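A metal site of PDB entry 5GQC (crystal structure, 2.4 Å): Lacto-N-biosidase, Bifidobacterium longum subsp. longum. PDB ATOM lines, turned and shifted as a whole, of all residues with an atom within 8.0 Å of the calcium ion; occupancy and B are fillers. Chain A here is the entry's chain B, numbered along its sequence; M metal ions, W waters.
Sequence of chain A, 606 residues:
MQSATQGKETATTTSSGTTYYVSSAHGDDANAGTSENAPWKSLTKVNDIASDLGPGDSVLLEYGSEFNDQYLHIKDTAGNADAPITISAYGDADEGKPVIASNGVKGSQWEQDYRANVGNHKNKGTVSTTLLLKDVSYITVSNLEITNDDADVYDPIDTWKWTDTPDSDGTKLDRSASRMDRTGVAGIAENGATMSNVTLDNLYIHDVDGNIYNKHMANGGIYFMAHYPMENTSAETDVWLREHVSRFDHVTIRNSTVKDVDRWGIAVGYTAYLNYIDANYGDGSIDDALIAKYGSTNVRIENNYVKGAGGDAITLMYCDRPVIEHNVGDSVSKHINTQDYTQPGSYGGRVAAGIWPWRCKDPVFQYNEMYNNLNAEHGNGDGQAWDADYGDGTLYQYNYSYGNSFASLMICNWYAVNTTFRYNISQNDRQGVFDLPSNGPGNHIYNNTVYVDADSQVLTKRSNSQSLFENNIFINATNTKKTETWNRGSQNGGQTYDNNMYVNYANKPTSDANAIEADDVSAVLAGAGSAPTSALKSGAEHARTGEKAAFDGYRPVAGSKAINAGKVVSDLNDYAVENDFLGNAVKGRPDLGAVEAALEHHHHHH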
ATOM      1  N   ASN A 103     -17.239  27.190 -13.206  1.00  0.00           N
ATOM      2  CA  ASN A 103     -16.062  28.043 -13.492  1.00  0.00           C
ATOM      3  C   ASN A 103     -14.706  27.444 -13.027  1.00  0.00           C
ATOM      4  O   ASN A 103     -13.695  28.159 -12.825  1.00  0.00           O
ATOM      5  CB  ASN A 103     -16.260  29.458 -12.957  1.00  0.00           C
ATOM      6  CG  ASN A 103     -17.412  30.206 -13.631  1.00  0.00           C
ATOM      7  OD1 ASN A 103     -17.684  30.055 -14.835  1.00  0.00           O
ATOM      8  ND2 ASN A 103     -18.080  31.033 -12.864  1.00  0.00           N
ATOM      9  N   ASN A 148     -18.692  24.793 -17.701  1.00  0.00           N
ATOM     10  CA  ASN A 148     -17.517  24.756 -16.859  1.00  0.00           C
ATOM     11  C   ASN A 148     -16.369  25.598 -17.484  1.00  0.00           C
ATOM     12  O   ASN A 148     -15.389  25.073 -18.045  1.00  0.00           O
ATOM     13  CB  ASN A 148     -17.086  23.328 -16.567  1.00  0.00           C
ATOM     14  CG  ASN A 148     -16.087  23.260 -15.444  1.00  0.00           C
ATOM     15  OD1 ASN A 148     -15.375  24.248 -15.174  1.00  0.00           O
ATOM     16  ND2 ASN A 148     -16.038  22.119 -14.744  1.00  0.00           N
ATOM     17  N   ASP A 149     -16.516  26.905 -17.283  1.00  0.00           N
ATOM     18  CA  ASP A 149     -15.835  27.961 -18.051  1.00  0.00           C
ATOM     19  C   ASP A 149     -14.596  28.533 -17.383  1.00  0.00           C
ATOM     20  O   ASP A 149     -14.502  28.569 -16.145  1.00  0.00           O
ATOM     21  CB  ASP A 149     -16.820  29.129 -18.293  1.00  0.00           C
ATOM     22  CG  ASP A 149     -16.415  30.026 -19.448  1.00  0.00           C
ATOM     23  OD1 ASP A 149     -15.805  29.544 -20.414  1.00  0.00           O
ATOM     24  OD2 ASP A 149     -16.697  31.222 -19.400  1.00  0.00           O
ATOM     25  N   ASP A 150     -13.666  28.961 -18.245  1.00  0.00           N
ATOM     26  CA  ASP A 150     -12.472  29.692 -17.900  1.00  0.00           C
ATOM     27  C   ASP A 150     -12.501  30.938 -18.754  1.00  0.00           C
ATOM     28  O   ASP A 150     -12.449  30.860 -19.975  1.00  0.00           O
ATOM     29  CB  ASP A 150     -11.217  28.890 -18.249  1.00  0.00           C
ATOM     30  CG  ASP A 150      -9.914  29.591 -17.823  1.00  0.00           C
ATOM     31  OD1 ASP A 150      -9.924  30.745 -17.350  1.00  0.00           O
ATOM     32  OD2 ASP A 150      -8.836  28.975 -17.955  1.00  0.00           O
ATOM     33  N   ALA A 151     -12.507  32.107 -18.114  1.00  0.00           N
ATOM     34  CA  ALA A 151     -12.640  33.333 -18.875  1.00  0.00           C
ATOM     35  C   ALA A 151     -11.349  33.684 -19.618  1.00  0.00           C
ATOM     36  O   ALA A 151     -11.363  34.574 -20.476  1.00  0.00           O
ATOM     37  CB  ALA A 151     -13.126  34.476 -17.988  1.00  0.00           C
ATOM     38  N   ASP A 152     -10.250  32.986 -19.299  1.00  0.00           N
ATOM     39  CA  ASP A 152      -9.003  33.050 -20.087  1.00  0.00           C
ATOM     40  C   ASP A 152      -8.866  32.081 -21.287  1.00  0.00           C
ATOM     41  O   ASP A 152      -7.828  32.044 -21.942  1.00  0.00           O
ATOM     42  CB  ASP A 152      -7.774  32.928 -19.178  1.00  0.00           C
ATOM     43  CG  ASP A 152      -6.938  34.212 -19.164  1.00  0.00           C
ATOM     44  OD1 ASP A 152      -6.401  34.580 -20.241  1.00  0.00           O
ATOM     45  OD2 ASP A 152      -6.842  34.855 -18.101  1.00  0.00           O
ATOM     46  N   VAL A 153      -9.926  31.317 -21.572  1.00  0.00           N
ATOM     47  CA  VAL A 153     -10.058  30.535 -22.803  1.00  0.00           C
ATOM     48  C   VAL A 153     -11.295  30.891 -23.667  1.00  0.00           C
ATOM     49  O   VAL A 153     -12.440  30.930 -23.183  1.00  0.00           O
ATOM     50  CB  VAL A 153     -10.182  29.045 -22.476  1.00  0.00           C
ATOM     51  CG1 VAL A 153     -10.100  28.225 -23.751  1.00  0.00           C
ATOM     52  CG2 VAL A 153      -9.091  28.613 -21.475  1.00  0.00           C
ATOM     53  N   TYR A 154     -11.112  31.076 -24.961  1.00  0.00           N
ATOM     54  CA  TYR A 154     -12.250  31.457 -25.793  1.00  0.00           C
ATOM     55  C   TYR A 154     -11.953  31.105 -27.241  1.00  0.00           C
ATOM     56  O   TYR A 154     -11.097  31.725 -27.880  1.00  0.00           O
ATOM     57  CB  TYR A 154     -12.577  32.963 -25.584  1.00  0.00           C
ATOM     58  CG  TYR A 154     -13.764  33.534 -26.367  1.00  0.00           C
ATOM     59  CD1 TYR A 154     -15.085  33.278 -25.979  1.00  0.00           C
ATOM     60  CD2 TYR A 154     -13.557  34.366 -27.487  1.00  0.00           C
ATOM     61  CE1 TYR A 154     -16.158  33.794 -26.699  1.00  0.00           C
ATOM     62  CE2 TYR A 154     -14.621  34.888 -28.218  1.00  0.00           C
ATOM     63  CZ  TYR A 154     -15.910  34.607 -27.816  1.00  0.00           C
ATOM     64  OH  TYR A 154     -16.964  35.114 -28.546  1.00  0.00           O
ATOM     65  N   ASP A 155     -12.642  30.067 -27.741  1.00  0.00           N
ATOM     66  CA  ASP A 155     -12.496  29.615 -29.128  1.00  0.00           C
ATOM     67  C   ASP A 155     -13.873  29.094 -29.578  1.00  0.00           C
ATOM     68  O   ASP A 155     -14.063  27.902 -29.734  1.00  0.00           O
ATOM     69  CB  ASP A 155     -11.400  28.543 -29.197  1.00  0.00           C
ATOM     70  CG  ASP A 155     -10.755  28.395 -30.557  1.00  0.00           C
ATOM     71  OD1 ASP A 155     -11.043  29.200 -31.501  1.00  0.00           O
ATOM     72  OD2 ASP A 155      -9.926  27.459 -30.690  1.00  0.00           O
ATOM     73  N   PRO A 156     -14.862  30.000 -29.724  1.00  0.00           N
ATOM     74  CA  PRO A 156     -16.184  29.552 -30.114  1.00  0.00           C
ATOM     75  C   PRO A 156     -16.222  28.934 -31.535  1.00  0.00           C
ATOM     76  O   PRO A 156     -15.643  29.493 -32.472  1.00  0.00           O
ATOM     77  CB  PRO A 156     -17.028  30.830 -30.070  1.00  0.00           C
ATOM     78  CG  PRO A 156     -16.043  31.931 -30.216  1.00  0.00           C
ATOM     79  CD  PRO A 156     -14.825  31.459 -29.485  1.00  0.00           C
ATOM     80  N   LYS A 172      -8.278  32.661 -27.738  1.00  0.00           N
ATOM     81  CA  LYS A 172      -7.216  32.347 -26.787  1.00  0.00           C
ATOM     82  C   LYS A 172      -7.384  30.993 -26.134  1.00  0.00           C
ATOM     83  O   LYS A 172      -8.419  30.690 -25.544  1.00  0.00           O
ATOM     84  CB  LYS A 172      -7.130  33.401 -25.697  1.00  0.00           C
ATOM     85  CG  LYS A 172      -5.876  33.299 -24.865  1.00  0.00           C
ATOM     86  CD  LYS A 172      -5.704  34.517 -23.963  1.00  0.00           C
ATOM     87  CE  LYS A 172      -4.754  34.237 -22.812  1.00  0.00           C
ATOM     88  NZ  LYS A 172      -3.358  33.911 -23.254  1.00  0.00           N
ATOM     89  N   ARG A 179      -2.880  21.169 -18.120  1.00  0.00           N
ATOM     90  CA  ARG A 179      -4.103  21.906 -17.807  1.00  0.00           C
ATOM     91  C   ARG A 179      -5.088  21.004 -17.085  1.00  0.00           C
ATOM     92  O   ARG A 179      -5.196  19.801 -17.433  1.00  0.00           O
ATOM     93  CB  ARG A 179      -4.795  22.417 -19.103  1.00  0.00           C
ATOM     94  CG  ARG A 179      -6.061  23.226 -18.857  1.00  0.00           C
ATOM     95  CD  ARG A 179      -6.614  23.834 -20.129  1.00  0.00           C
ATOM     96  NE  ARG A 179      -7.878  24.492 -19.812  1.00  0.00           N
ATOM     97  CZ  ARG A 179      -8.010  25.685 -19.241  1.00  0.00           C
ATOM     98  NH1 ARG A 179      -6.956  26.429 -18.980  1.00  0.00           N
ATOM     99  NH2 ARG A 179      -9.217  26.126 -18.931  1.00  0.00           N
ATOM    100  N   ARG A 182     -11.467  19.253 -17.203  1.00  0.00           N
ATOM    101  CA  ARG A 182     -12.868  19.655 -16.844  1.00  0.00           C
ATOM    102  C   ARG A 182     -13.988  18.890 -17.516  1.00  0.00           C
ATOM    103  O   ARG A 182     -13.943  18.580 -18.706  1.00  0.00           O
ATOM    104  CB  ARG A 182     -13.103  21.120 -17.127  1.00  0.00           C
ATOM    105  CG  ARG A 182     -12.085  21.996 -16.459  1.00  0.00           C
ATOM    106  CD  ARG A 182     -12.645  23.374 -16.431  1.00  0.00           C
ATOM    107  NE  ARG A 182     -11.622  24.373 -16.192  1.00  0.00           N
ATOM    108  CZ  ARG A 182     -11.878  25.618 -15.828  1.00  0.00           C
ATOM    109  NH1 ARG A 182     -13.161  26.006 -15.683  1.00  0.00           N
ATOM    110  NH2 ARG A 182     -10.886  26.478 -15.625  1.00  0.00           N
ATOM    111  N   ASP A 207     -19.205  25.541 -23.121  1.00  0.00           N
ATOM    112  CA  ASP A 207     -18.066  26.219 -22.545  1.00  0.00           C
ATOM    113  C   ASP A 207     -17.451  25.429 -21.355  1.00  0.00           C
ATOM    114  O   ASP A 207     -17.242  25.954 -20.282  1.00  0.00           O
ATOM    115  CB  ASP A 207     -18.431  27.661 -22.225  1.00  0.00           C
ATOM    116  CG  ASP A 207     -18.785  28.459 -23.486  1.00  0.00           C
ATOM    117  OD1 ASP A 207     -17.859  28.747 -24.257  1.00  0.00           O
ATOM    118  OD2 ASP A 207     -19.964  28.809 -23.725  1.00  0.00           O
ATOM    119  N   VAL A 208     -17.173  24.150 -21.613  1.00  0.00           N
ATOM    120  CA  VAL A 208     -16.345  23.334 -20.773  1.00  0.00           C
ATOM    121  C   VAL A 208     -14.918  23.450 -21.284  1.00  0.00           C
ATOM    122  O   VAL A 208     -14.511  22.729 -22.184  1.00  0.00           O
ATOM    123  CB  VAL A 208     -16.748  21.857 -20.805  1.00  0.00           C
ATOM    124  CG1 VAL A 208     -15.862  21.071 -19.836  1.00  0.00           C
ATOM    125  CG2 VAL A 208     -18.223  21.693 -20.472  1.00  0.00           C
ATOM    126  N   ASP A 209     -14.136  24.321 -20.669  1.00  0.00           N
ATOM    127  CA  ASP A 209     -12.758  24.500 -21.081  1.00  0.00           C
ATOM    128  C   ASP A 209     -11.799  23.536 -20.339  1.00  0.00           C
ATOM    129  O   ASP A 209     -11.040  23.914 -19.460  1.00  0.00           O
ATOM    130  CB  ASP A 209     -12.404  25.963 -20.940  1.00  0.00           C
ATOM    131  CG  ASP A 209     -13.337  26.870 -21.748  1.00  0.00           C
ATOM    132  OD1 ASP A 209     -13.838  26.443 -22.856  1.00  0.00           O
ATOM    133  OD2 ASP A 209     -13.609  28.012 -21.255  1.00  0.00           O
ATOM    134  N   ASP A 260     -18.770  23.583 -27.743  1.00  0.00           N
ATOM    135  CA  ASP A 260     -17.566  24.314 -27.303  1.00  0.00           C
ATOM    136  C   ASP A 260     -16.981  23.709 -26.024  1.00  0.00           C
ATOM    137  O   ASP A 260     -16.857  24.356 -24.975  1.00  0.00           O
ATOM    138  CB  ASP A 260     -17.864  25.824 -27.109  1.00  0.00           C
ATOM    139  CG  ASP A 260     -18.003  26.570 -28.411  1.00  0.00           C
ATOM    140  OD1 ASP A 260     -17.439  26.120 -29.456  1.00  0.00           O
ATOM    141  OD2 ASP A 260     -18.669  27.632 -28.386  1.00  0.00           O
HETATM  142 CA    CA M   1     -14.050  30.352 -21.848  1.00  0.00          CA
HETATM  143  O   HOH W   1     -15.146  28.739 -24.079  1.00  0.00           O
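Water W1 lies within hydrogen-bond range of OD1 of Asp 207 (2.7 Å) and OD1 of Asp 209 (2.9 Å).
Of the 17 residues printed, 4 come within 4 Å of the calcium ion. Along chain A the residues within 4 Å of the calcium ion span positions 149 to 209. The nearest printed residue that does not touch the calcium ion is Tyr 154 (4.3 Å).
The backbone carbonyl oxygen (O) of Val 153 binds the calcium ion. The side-chain carboxylate (OD1) of Asp 149 binds the calcium ion. The calcium ion is bound by OD2 of Asp 209, 2.5 Å away. The backbone carbonyl oxygen (O) of Asp 150 binds the calcium ion, at 2.5 Å. The calcium ion has four donor atoms within binding distance. Slightly farther from the calcium ion lies water W1 (3.0 Å).
The backbone NH (N) of Asp 149 lies within hydrogen-bond range of the backbone carbonyl oxygen (O) of Asp 207, 3.2 Å away. The backbone NH (N) of Asp 209 lies within hydrogen-bond range of the backbone carbonyl oxygen (O) of Asn 148 (3.0 Å). NH2 of Arg 182 lies within salt-bridge range of OD2 of Asp 150 (3.98 Å). O of Asp 209 sits at hydrogen-bond distance from NE of Arg 182, at 3.4 Å. The guanidinium group (NH2) of Arg 179 is in salt-bridge range of the side-chain carboxylate (OD2) of Asp 150, at 3.0 Å. The guanidinium group of Arg 182 sits at hydrogen-bond distance from the backbone carbonyl oxygen of Asp 149. O of Asp 209 sits at hydrogen-bond distance from NH2 of Arg 179, 2.9 Å away. The side-chain carboxylate (OD1) of Asp 150 lies within hydrogen-bond range of the backbone NH (N) of Asp 152, at 3.0 Å.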
